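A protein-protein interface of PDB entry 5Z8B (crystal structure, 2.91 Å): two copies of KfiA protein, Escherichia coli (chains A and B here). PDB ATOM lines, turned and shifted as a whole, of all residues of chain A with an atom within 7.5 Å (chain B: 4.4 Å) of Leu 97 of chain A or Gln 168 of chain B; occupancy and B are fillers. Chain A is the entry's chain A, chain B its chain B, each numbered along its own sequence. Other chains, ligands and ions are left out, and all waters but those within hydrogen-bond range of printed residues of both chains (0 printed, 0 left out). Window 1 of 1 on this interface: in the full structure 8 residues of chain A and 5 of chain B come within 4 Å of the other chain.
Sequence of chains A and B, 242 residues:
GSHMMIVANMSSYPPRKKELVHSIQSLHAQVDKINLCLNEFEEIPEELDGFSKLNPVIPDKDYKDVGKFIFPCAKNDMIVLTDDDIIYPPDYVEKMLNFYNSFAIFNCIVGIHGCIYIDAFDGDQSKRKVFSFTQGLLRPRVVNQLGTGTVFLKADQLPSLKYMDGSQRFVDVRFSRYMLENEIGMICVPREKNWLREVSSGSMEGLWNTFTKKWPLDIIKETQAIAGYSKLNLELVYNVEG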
ATOM      1  N   ILE A   6      21.186   8.522  -2.741  1.00  0.00           N
ATOM      2  CA  ILE A   6      20.689   8.768  -4.115  1.00  0.00           C
ATOM      3  C   ILE A   6      19.364   9.510  -4.037  1.00  0.00           C
ATOM      4  O   ILE A   6      18.385   8.958  -3.532  1.00  0.00           O
ATOM      5  CB  ILE A   6      20.396   7.451  -4.907  1.00  0.00           C
ATOM      6  CG1 ILE A   6      21.631   6.538  -5.014  1.00  0.00           C
ATOM      7  CG2 ILE A   6      19.806   7.770  -6.283  1.00  0.00           C
ATOM      8  CD1 ILE A   6      22.821   7.136  -5.714  1.00  0.00           C
ATOM      9  N   ASP A  32      16.911   6.698  -2.768  1.00  0.00           N
ATOM     10  CA  ASP A  32      16.768   6.818  -1.306  1.00  0.00           C
ATOM     11  C   ASP A  32      15.752   7.864  -0.858  1.00  0.00           C
ATOM     12  O   ASP A  32      15.451   7.945   0.332  1.00  0.00           O
ATOM     13  CB  ASP A  32      18.126   7.106  -0.647  1.00  0.00           C
ATOM     14  CG  ASP A  32      19.097   5.937  -0.771  1.00  0.00           C
ATOM     15  OD1 ASP A  32      18.771   4.845  -0.263  1.00  0.00           O
ATOM     16  OD2 ASP A  32      20.192   6.104  -1.371  1.00  0.00           O
ATOM     17  N   MET A  78      23.964  12.140  -4.597  1.00  0.00           N
ATOM     18  CA  MET A  78      23.907  11.985  -6.025  1.00  0.00           C
ATOM     19  C   MET A  78      22.475  12.284  -6.420  1.00  0.00           C
ATOM     20  O   MET A  78      21.553  11.631  -5.951  1.00  0.00           O
ATOM     21  CB  MET A  78      24.281  10.563  -6.424  1.00  0.00           C
ATOM     22  CG  MET A  78      25.782  10.253  -6.364  1.00  0.00           C
ATOM     23  SD  MET A  78      26.883  11.062  -7.578  1.00  0.00           S
ATOM     24  CE  MET A  78      25.984  11.020  -9.134  1.00  0.00           C
ATOM     25  N   ASP A  91      16.753  -0.922 -13.529  1.00  0.00           N
ATOM     26  CA  ASP A  91      18.217  -0.794 -13.360  1.00  0.00           C
ATOM     27  C   ASP A  91      18.712   0.612 -13.743  1.00  0.00           C
ATOM     28  O   ASP A  91      19.893   0.808 -14.063  1.00  0.00           O
ATOM     29  CB  ASP A  91      18.929  -1.844 -14.253  1.00  0.00           C
ATOM     30  CG  ASP A  91      18.573  -1.702 -15.779  1.00  0.00           C
ATOM     31  OD1 ASP A  91      17.521  -1.098 -16.112  1.00  0.00           O
ATOM     32  OD2 ASP A  91      19.333  -2.205 -16.640  1.00  0.00           O
ATOM     33  N   TYR A  92      17.807   1.594 -13.729  1.00  0.00           N
ATOM     34  CA  TYR A  92      18.153   2.951 -14.093  1.00  0.00           C
ATOM     35  C   TYR A  92      19.294   3.450 -13.214  1.00  0.00           C
ATOM     36  O   TYR A  92      20.330   3.765 -13.727  1.00  0.00           O
ATOM     37  CB  TYR A  92      16.933   3.856 -13.996  1.00  0.00           C
ATOM     38  CG  TYR A  92      17.165   5.243 -14.541  1.00  0.00           C
ATOM     39  CD1 TYR A  92      17.449   5.437 -15.884  1.00  0.00           C
ATOM     40  CD2 TYR A  92      17.108   6.354 -13.721  1.00  0.00           C
ATOM     41  CE1 TYR A  92      17.672   6.698 -16.395  1.00  0.00           C
ATOM     42  CE2 TYR A  92      17.337   7.621 -14.219  1.00  0.00           C
ATOM     43  CZ  TYR A  92      17.615   7.794 -15.560  1.00  0.00           C
ATOM     44  OH  TYR A  92      17.826   9.066 -16.075  1.00  0.00           O
ATOM     45  N   VAL A  93      19.125   3.450 -11.895  1.00  0.00           N
ATOM     46  CA  VAL A  93      20.127   4.021 -10.975  1.00  0.00           C
ATOM     47  C   VAL A  93      21.437   3.232 -10.979  1.00  0.00           C
ATOM     48  O   VAL A  93      22.504   3.826 -11.107  1.00  0.00           O
ATOM     49  CB  VAL A  93      19.593   4.153  -9.521  1.00  0.00           C
ATOM     50  CG1 VAL A  93      20.699   4.571  -8.559  1.00  0.00           C
ATOM     51  CG2 VAL A  93      18.438   5.147  -9.438  1.00  0.00           C
ATOM     52  N   GLU A  94      21.362   1.909 -10.828  1.00  0.00           N
ATOM     53  CA  GLU A  94      22.547   1.038 -10.990  1.00  0.00           C
ATOM     54  C   GLU A  94      23.364   1.423 -12.246  1.00  0.00           C
ATOM     55  O   GLU A  94      24.543   1.732 -12.139  1.00  0.00           O
ATOM     56  CB  GLU A  94      22.132  -0.438 -11.049  1.00  0.00           C
ATOM     57  CG  GLU A  94      23.260  -1.449 -11.250  1.00  0.00           C
ATOM     58  CD  GLU A  94      22.770  -2.892 -11.491  1.00  0.00           C
ATOM     59  OE1 GLU A  94      22.921  -3.724 -10.563  1.00  0.00           O
ATOM     60  OE2 GLU A  94      22.249  -3.215 -12.595  1.00  0.00           O
ATOM     61  N   LYS A  95      22.727   1.424 -13.412  1.00  0.00           N
ATOM     62  CA  LYS A  95      23.423   1.669 -14.674  1.00  0.00           C
ATOM     63  C   LYS A  95      24.036   3.046 -14.747  1.00  0.00           C
ATOM     64  O   LYS A  95      25.210   3.193 -15.119  1.00  0.00           O
ATOM     65  CB  LYS A  95      22.488   1.511 -15.869  1.00  0.00           C
ATOM     66  CG  LYS A  95      22.197   0.071 -16.245  1.00  0.00           C
ATOM     67  CD  LYS A  95      23.321  -0.542 -17.083  1.00  0.00           C
ATOM     68  CE  LYS A  95      22.905  -1.865 -17.716  1.00  0.00           C
ATOM     69  NZ  LYS A  95      22.625  -2.915 -16.690  1.00  0.00           N
ATOM     70  N   MET A  96      23.231   4.048 -14.414  1.00  0.00           N
ATOM     71  CA  MET A  96      23.626   5.450 -14.532  1.00  0.00           C
ATOM     72  C   MET A  96      24.776   5.796 -13.590  1.00  0.00           C
ATOM     73  O   MET A  96      25.689   6.501 -13.980  1.00  0.00           O
ATOM     74  CB  MET A  96      22.418   6.383 -14.293  1.00  0.00           C
ATOM     75  CG  MET A  96      21.334   6.307 -15.368  1.00  0.00           C
ATOM     76  SD  MET A  96      21.857   6.993 -16.965  1.00  0.00           S
ATOM     77  CE  MET A  96      21.403   8.710 -16.759  1.00  0.00           C
ATOM     78  N   LEU A  97      24.715   5.287 -12.359  1.00  0.00           N
ATOM     79  CA  LEU A  97      25.776   5.478 -11.365  1.00  0.00           C
ATOM     80  C   LEU A  97      27.092   4.925 -11.888  1.00  0.00           C
ATOM     81  O   LEU A  97      28.123   5.581 -11.734  1.00  0.00           O
ATOM     82  CB  LEU A  97      25.430   4.804 -10.030  1.00  0.00           C
ATOM     83  CG  LEU A  97      25.917   5.436  -8.718  1.00  0.00           C
ATOM     84  CD1 LEU A  97      25.860   4.394  -7.607  1.00  0.00           C
ATOM     85  CD2 LEU A  97      27.326   6.023  -8.780  1.00  0.00           C
ATOM     86  N   ASN A  98      27.051   3.741 -12.512  1.00  0.00           N
ATOM     87  CA  ASN A  98      28.262   3.117 -13.071  1.00  0.00           C
ATOM     88  C   ASN A  98      28.796   3.886 -14.269  1.00  0.00           C
ATOM     89  O   ASN A  98      30.012   4.011 -14.421  1.00  0.00           O
ATOM     90  CB  ASN A  98      28.057   1.634 -13.407  1.00  0.00           C
ATOM     91  CG  ASN A  98      28.470   0.717 -12.260  1.00  0.00           C
ATOM     92  OD1 ASN A  98      29.637   0.370 -12.142  1.00  0.00           O
ATOM     93  ND2 ASN A  98      27.516   0.345 -11.394  1.00  0.00           N
ATOM     94  N   PHE A  99      27.906   4.443 -15.089  1.00  0.00           N
ATOM     95  CA  PHE A  99      28.344   5.382 -16.124  1.00  0.00           C
ATOM     96  C   PHE A  99      29.042   6.571 -15.493  1.00  0.00           C
ATOM     97  O   PHE A  99      30.173   6.893 -15.875  1.00  0.00           O
ATOM     98  CB  PHE A  99      27.190   5.842 -17.026  1.00  0.00           C
ATOM     99  CG  PHE A  99      26.665   4.758 -17.942  1.00  0.00           C
ATOM    100  CD1 PHE A  99      27.539   3.988 -18.729  1.00  0.00           C
ATOM    101  CD2 PHE A  99      25.303   4.501 -18.032  1.00  0.00           C
ATOM    102  CE1 PHE A  99      27.056   2.986 -19.555  1.00  0.00           C
ATOM    103  CE2 PHE A  99      24.822   3.495 -18.862  1.00  0.00           C
ATOM    104  CZ  PHE A  99      25.696   2.737 -19.617  1.00  0.00           C
ATOM    105  N   TYR A 100      28.388   7.190 -14.508  1.00  0.00           N
ATOM    106  CA  TYR A 100      28.946   8.347 -13.810  1.00  0.00           C
ATOM    107  C   TYR A 100      30.293   8.042 -13.169  1.00  0.00           C
ATOM    108  O   TYR A 100      31.202   8.835 -13.300  1.00  0.00           O
ATOM    109  CB  TYR A 100      27.995   8.898 -12.750  1.00  0.00           C
ATOM    110  CG  TYR A 100      28.459  10.223 -12.177  1.00  0.00           C
ATOM    111  CD1 TYR A 100      29.358  10.265 -11.133  1.00  0.00           C
ATOM    112  CD2 TYR A 100      28.005  11.434 -12.700  1.00  0.00           C
ATOM    113  CE1 TYR A 100      29.781  11.472 -10.605  1.00  0.00           C
ATOM    114  CE2 TYR A 100      28.428  12.651 -12.191  1.00  0.00           C
ATOM    115  CZ  TYR A 100      29.316  12.668 -11.137  1.00  0.00           C
ATOM    116  OH  TYR A 100      29.773  13.856 -10.611  1.00  0.00           O
ATOM    117  N   ASN A 101      30.428   6.905 -12.501  1.00  0.00           N
ATOM    118  CA  ASN A 101      31.698   6.561 -11.843  1.00  0.00           C
ATOM    119  C   ASN A 101      32.808   6.133 -12.805  1.00  0.00           C
ATOM    120  O   ASN A 101      33.952   6.543 -12.621  1.00  0.00           O
ATOM    121  CB  ASN A 101      31.488   5.484 -10.781  1.00  0.00           C
ATOM    122  CG  ASN A 101      30.795   6.013  -9.543  1.00  0.00           C
ATOM    123  OD1 ASN A 101      30.614   7.216  -9.386  1.00  0.00           O
ATOM    124  ND2 ASN A 101      30.406   5.113  -8.655  1.00  0.00           N
ATOM    125  N   SER A 102      32.482   5.309 -13.800  1.00  0.00           N
ATOM    126  CA  SER A 102      33.421   4.979 -14.890  1.00  0.00           C
ATOM    127  C   SER A 102      33.903   6.203 -15.651  1.00  0.00           C
ATOM    128  O   SER A 102      35.094   6.335 -15.914  1.00  0.00           O
ATOM    129  CB  SER A 102      32.759   4.066 -15.916  1.00  0.00           C
ATOM    130  OG  SER A 102      32.300   2.890 -15.297  1.00  0.00           O
ATOM    131  N   PHE A 103      32.970   7.083 -16.009  1.00  0.00           N
ATOM    132  CA  PHE A 103      33.286   8.247 -16.823  1.00  0.00           C
ATOM    133  C   PHE A 103      33.843   9.426 -16.036  1.00  0.00           C
ATOM    134  O   PHE A 103      34.234  10.400 -16.637  1.00  0.00           O
ATOM    135  CB  PHE A 103      32.059   8.688 -17.630  1.00  0.00           C
ATOM    136  CG  PHE A 103      31.497   7.619 -18.554  1.00  0.00           C
ATOM    137  CD1 PHE A 103      32.292   6.580 -19.070  1.00  0.00           C
ATOM    138  CD2 PHE A 103      30.166   7.672 -18.954  1.00  0.00           C
ATOM    139  CE1 PHE A 103      31.757   5.621 -19.933  1.00  0.00           C
ATOM    140  CE2 PHE A 103      29.638   6.704 -19.813  1.00  0.00           C
ATOM    141  CZ  PHE A 103      30.435   5.679 -20.304  1.00  0.00           C
ATOM    142  N   VAL A 110      26.400  12.975 -16.562  1.00  0.00           N
ATOM    143  CA  VAL A 110      25.949  11.959 -17.525  1.00  0.00           C
ATOM    144  C   VAL A 110      24.475  12.161 -17.720  1.00  0.00           C
ATOM    145  O   VAL A 110      23.827  12.636 -16.803  1.00  0.00           O
ATOM    146  CB  VAL A 110      26.232  10.464 -17.100  1.00  0.00           C
ATOM    147  CG1 VAL A 110      27.719  10.153 -17.192  1.00  0.00           C
ATOM    148  CG2 VAL A 110      25.693  10.076 -15.715  1.00  0.00           C
ATOM    149  N   PHE A 152      22.176  12.697 -14.277  1.00  0.00           N
ATOM    150  CA  PHE A 152      22.730  12.149 -13.075  1.00  0.00           C
ATOM    151  C   PHE A 152      23.994  12.928 -12.679  1.00  0.00           C
ATOM    152  O   PHE A 152      24.916  13.084 -13.480  1.00  0.00           O
ATOM    153  CB  PHE A 152      23.049  10.703 -13.366  1.00  0.00           C
ATOM    154  CG  PHE A 152      22.864   9.816 -12.210  1.00  0.00           C
ATOM    155  CD1 PHE A 152      23.871   9.699 -11.255  1.00  0.00           C
ATOM    156  CD2 PHE A 152      21.694   9.094 -12.071  1.00  0.00           C
ATOM    157  CE1 PHE A 152      23.721   8.871 -10.169  1.00  0.00           C
ATOM    158  CE2 PHE A 152      21.531   8.259 -10.988  1.00  0.00           C
ATOM    159  CZ  PHE A 152      22.548   8.149 -10.036  1.00  0.00           C
ATOM    160  N   TYR B  63      22.310  -0.877   4.373  1.00  0.00           N
ATOM    161  CA  TYR B  63      23.538  -1.167   3.652  1.00  0.00           C
ATOM    162  C   TYR B  63      23.385  -1.760   2.254  1.00  0.00           C
ATOM    163  O   TYR B  63      24.373  -1.889   1.565  1.00  0.00           O
ATOM    164  CB  TYR B  63      24.385  -2.099   4.492  1.00  0.00           C
ATOM    165  CG  TYR B  63      24.998  -1.430   5.679  1.00  0.00           C
ATOM    166  CD1 TYR B  63      26.086  -0.578   5.527  1.00  0.00           C
ATOM    167  CD2 TYR B  63      24.519  -1.657   6.951  1.00  0.00           C
ATOM    168  CE1 TYR B  63      26.668   0.049   6.620  1.00  0.00           C
ATOM    169  CE2 TYR B  63      25.096  -1.044   8.050  1.00  0.00           C
ATOM    170  CZ  TYR B  63      26.167  -0.191   7.874  1.00  0.00           C
ATOM    171  OH  TYR B  63      26.741   0.420   8.937  1.00  0.00           O
ATOM    172  N   LYS B  64      22.172  -2.125   1.834  1.00  0.00           N
ATOM    173  CA  LYS B  64      21.927  -2.744   0.506  1.00  0.00           C
ATOM    174  C   LYS B  64      22.899  -3.898   0.200  1.00  0.00           C
ATOM    175  O   LYS B  64      23.112  -4.728   1.057  1.00  0.00           O
ATOM    176  CB  LYS B  64      21.932  -1.681  -0.595  1.00  0.00           C
ATOM    177  CG  LYS B  64      20.831  -0.672  -0.424  1.00  0.00           C
ATOM    178  CD  LYS B  64      21.169   0.651  -1.096  1.00  0.00           C
ATOM    179  CE  LYS B  64      20.521   1.796  -0.328  1.00  0.00           C
ATOM    180  NZ  LYS B  64      19.041   1.606  -0.327  1.00  0.00           N
ATOM    181  N   ASP B  65      23.501  -3.939  -0.990  1.00  0.00           N
ATOM    182  CA  ASP B  65      24.387  -5.055  -1.407  1.00  0.00           C
ATOM    183  C   ASP B  65      25.715  -5.106  -0.598  1.00  0.00           C
ATOM    184  O   ASP B  65      26.366  -6.153  -0.556  1.00  0.00           O
ATOM    185  CB  ASP B  65      24.596  -5.133  -2.972  1.00  0.00           C
ATOM    186  CG  ASP B  65      24.682  -3.710  -3.718  1.00  0.00           C
ATOM    187  OD1 ASP B  65      24.485  -2.602  -3.103  1.00  0.00           O
ATOM    188  OD2 ASP B  65      24.957  -3.723  -4.963  1.00  0.00           O
ATOM    189  N   VAL B  66      26.068  -3.987   0.047  1.00  0.00           N
ATOM    190  CA  VAL B  66      27.151  -3.908   1.042  1.00  0.00           C
ATOM    191  C   VAL B  66      26.829  -4.626   2.381  1.00  0.00           C
ATOM    192  O   VAL B  66      27.751  -5.055   3.102  1.00  0.00           O
ATOM    193  CB  VAL B  66      27.565  -2.421   1.303  1.00  0.00           C
ATOM    194  CG1 VAL B  66      28.559  -2.255   2.460  1.00  0.00           C
ATOM    195  CG2 VAL B  66      28.147  -1.806   0.035  1.00  0.00           C
ATOM    196  N   ASP B 165      31.937   0.649   2.385  1.00  0.00           N
ATOM    197  CA  ASP B 165      30.808   1.600   2.474  1.00  0.00           C
ATOM    198  C   ASP B 165      30.940   2.702   1.410  1.00  0.00           C
ATOM    199  O   ASP B 165      32.043   3.077   1.009  1.00  0.00           O
ATOM    200  CB  ASP B 165      30.633   2.196   3.890  1.00  0.00           C
ATOM    201  CG  ASP B 165      29.134   2.491   4.252  1.00  0.00           C
ATOM    202  OD1 ASP B 165      28.197   2.196   3.447  1.00  0.00           O
ATOM    203  OD2 ASP B 165      28.910   3.012   5.376  1.00  0.00           O
ATOM    204  N   GLY B 166      29.796   3.170   0.926  1.00  0.00           N
ATOM    205  CA  GLY B 166      29.742   4.047  -0.234  1.00  0.00           C
ATOM    206  C   GLY B 166      29.601   3.296  -1.545  1.00  0.00           C
ATOM    207  O   GLY B 166      29.154   3.879  -2.535  1.00  0.00           O
ATOM    208  N   SER B 167      29.904   1.998  -1.562  1.00  0.00           N
ATOM    209  CA  SER B 167      29.946   1.238  -2.811  1.00  0.00           C
ATOM    210  C   SER B 167      28.600   0.668  -3.281  1.00  0.00           C
ATOM    211  O   SER B 167      28.581  -0.235  -4.125  1.00  0.00           O
ATOM    212  CB  SER B 167      30.962   0.102  -2.691  1.00  0.00           C
ATOM    213  OG  SER B 167      30.489  -0.923  -1.825  1.00  0.00           O
ATOM    214  N   GLN B 168      27.487   1.212  -2.786  1.00  0.00           N
ATOM    215  CA  GLN B 168      26.174   0.605  -3.027  1.00  0.00           C
ATOM    216  C   GLN B 168      25.784   0.756  -4.481  1.00  0.00           C
ATOM    217  O   GLN B 168      26.005   1.802  -5.095  1.00  0.00           O
ATOM    218  CB  GLN B 168      25.085   1.191  -2.117  1.00  0.00           C
ATOM    219  CG  GLN B 168      25.097   0.677  -0.683  1.00  0.00           C
ATOM    220  CD  GLN B 168      26.186   1.287   0.180  1.00  0.00           C
ATOM    221  OE1 GLN B 168      27.127   1.916  -0.314  1.00  0.00           O
ATOM    222  NE2 GLN B 168      26.064   1.091   1.498  1.00  0.00           N
ATOM    223  N   ARG B 169      25.246  -0.322  -5.028  1.00  0.00           N
ATOM    224  CA  ARG B 169      24.871  -0.412  -6.433  1.00  0.00           C
ATOM    225  C   ARG B 169      26.075  -0.460  -7.422  1.00  0.00           C
ATOM    226  O   ARG B 169      25.873  -0.566  -8.661  1.00  0.00           O
ATOM    227  CB  ARG B 169      23.848   0.680  -6.800  1.00  0.00           C
ATOM    228  CG  ARG B 169      22.681   0.831  -5.815  1.00  0.00           C
ATOM    229  CD  ARG B 169      21.792   2.021  -6.180  1.00  0.00           C
ATOM    230  NE  ARG B 169      20.980   2.570  -5.077  1.00  0.00           N
ATOM    231  CZ  ARG B 169      21.445   3.296  -4.049  1.00  0.00           C
ATOM    232  NH1 ARG B 169      20.597   3.763  -3.127  1.00  0.00           N
ATOM    233  NH2 ARG B 169      22.750   3.566  -3.920  1.00  0.00           N
ATOM    234  N   PHE B 170      27.306  -0.395  -6.887  1.00  0.00           N
ATOM    235  CA  PHE B 170      28.517  -0.778  -7.629  1.00  0.00           C
ATOM    236  C   PHE B 170      29.499  -1.569  -6.744  1.00  0.00           C
ATOM    237  O   PHE B 170      30.705  -1.454  -6.887  1.00  0.00           O
ATOM    238  CB  PHE B 170      29.173   0.459  -8.302  1.00  0.00           C
ATOM    239  CG  PHE B 170      29.768   1.461  -7.343  1.00  0.00           C
ATOM    240  CD1 PHE B 170      28.959   2.382  -6.682  1.00  0.00           C
ATOM    241  CD2 PHE B 170      31.144   1.506  -7.125  1.00  0.00           C
ATOM    242  CE1 PHE B 170      29.501   3.315  -5.807  1.00  0.00           C
ATOM    243  CE2 PHE B 170      31.694   2.439  -6.252  1.00  0.00           C
ATOM    244  CZ  PHE B 170      30.871   3.352  -5.594  1.00  0.00           C
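Among the printed residues, pairs that only touch across the chains: Ile 6 of chain A with Arg 169 of chain B (3.4 Å), Asn 101 of chain A with Phe 170 of chain B (3.5 Å), Asn 98 of chain A with Phe 170 of chain B (3.5 Å), Leu 97 of chain A with Gln 168 of chain B (3.6 Å), Val 93 of chain A with Arg 169 of chain B (3.7 Å), Glu 94 of chain A with Arg 169 of chain B (3.8 Å) and Leu 97 of chain A with Phe 170 of chain B (3.8 Å).
Printed residues of chain A that touch a printed residue of chain B: Ile 6, Asp 32, Val 93, Glu 94, Leu 97, Asn 98 and Asn 101.
Hydrophobic or aromatic side chains of chain A within 4 Å of the printed part of chain B: Ile 6, Val 93 and Leu 97.
Of the 10 printed residues of chain B, 4 touch a printed residue of chain A.
Among the printed residues, Asp or Glu carboxylates within 4 Å of a Lys or Arg side-chain nitrogen of the other chain: Asp 32 of chain A with Lys 64 of chain B (3.3 Å) and Asp 32 of chain A with Arg 169 of chain B (3.0 Å).
The side-chain amino group of Lys 64 of chain B lies within salt-bridge range of the side-chain carboxylate of Asp 32 of chain A, at 3.3 Å.
The side-chain carboxylate of Asp 32 of chain A is in salt-bridge range of the guanidinium group of Arg 169 of chain B (3.0 Å).
ND2 of Asn 98 of chain A lies within hydrogen-bond range of O of Arg 169 of chain B (3.3 Å).
Of chain B, only Gln 168 and Phe 170 come within 4 Å of Leu 97 of chain A.
Of chain A, only Leu 97 (3.6 Å) comes within 4 Å of Gln 168 of chain B.
Printed residues of chain B within 4 Å of Asn 98 of chain A: Arg 169 (3.3 Å) and Phe 170 (3.5 Å).
Of the printed residues of chain B, Val 93 of chain A touches Arg 169 (3.7 Å).
Of the printed residues of chain A, Lys 64 of chain B touches Asp 32 (3.3 Å).
Of the printed residues of chain B, Glu 94 of chain A touches Arg 169 (3.8 Å).
Of the printed residues of chain B, Asn 101 of chain A touches Phe 170 (3.5 Å).
The nearest residue of chain B that does not touch Leu 97 of chain A is Arg 169 of chain B (4.3 Å).
N of Asp 32 of chain A lies within hydrogen-bond range of O of Ile 6 of chain A (2.8 Å).
O of Glu 94 of chain A is in hydrogen-bond range of ND2 of Asn 98 of chain A (3.4 Å).
The backbone carbonyl oxygen (O) of Tyr 63 of chain B sits at hydrogen-bond distance from the side-chain amide nitrogen (NE2) of Gln 168 of chain B (3.4 Å).
N of Arg 169 of chain B is in hydrogen-bond range of OD1 of Asp 65 of chain B (3.1 Å).
OD1 of Asp 165 of chain B is in hydrogen-bond range of NE2 of Gln 168 of chain B.
The backbone NH (N) of Gly 166 of chain B lies close to the side-chain amide oxygen (OE1) of Gln 168 of chain B (3.2 Å).
No position is printed for both chains.
Of the 10 pairs that touch across the chains among the printed residues, none has its exchanged pair printed and touching as well.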
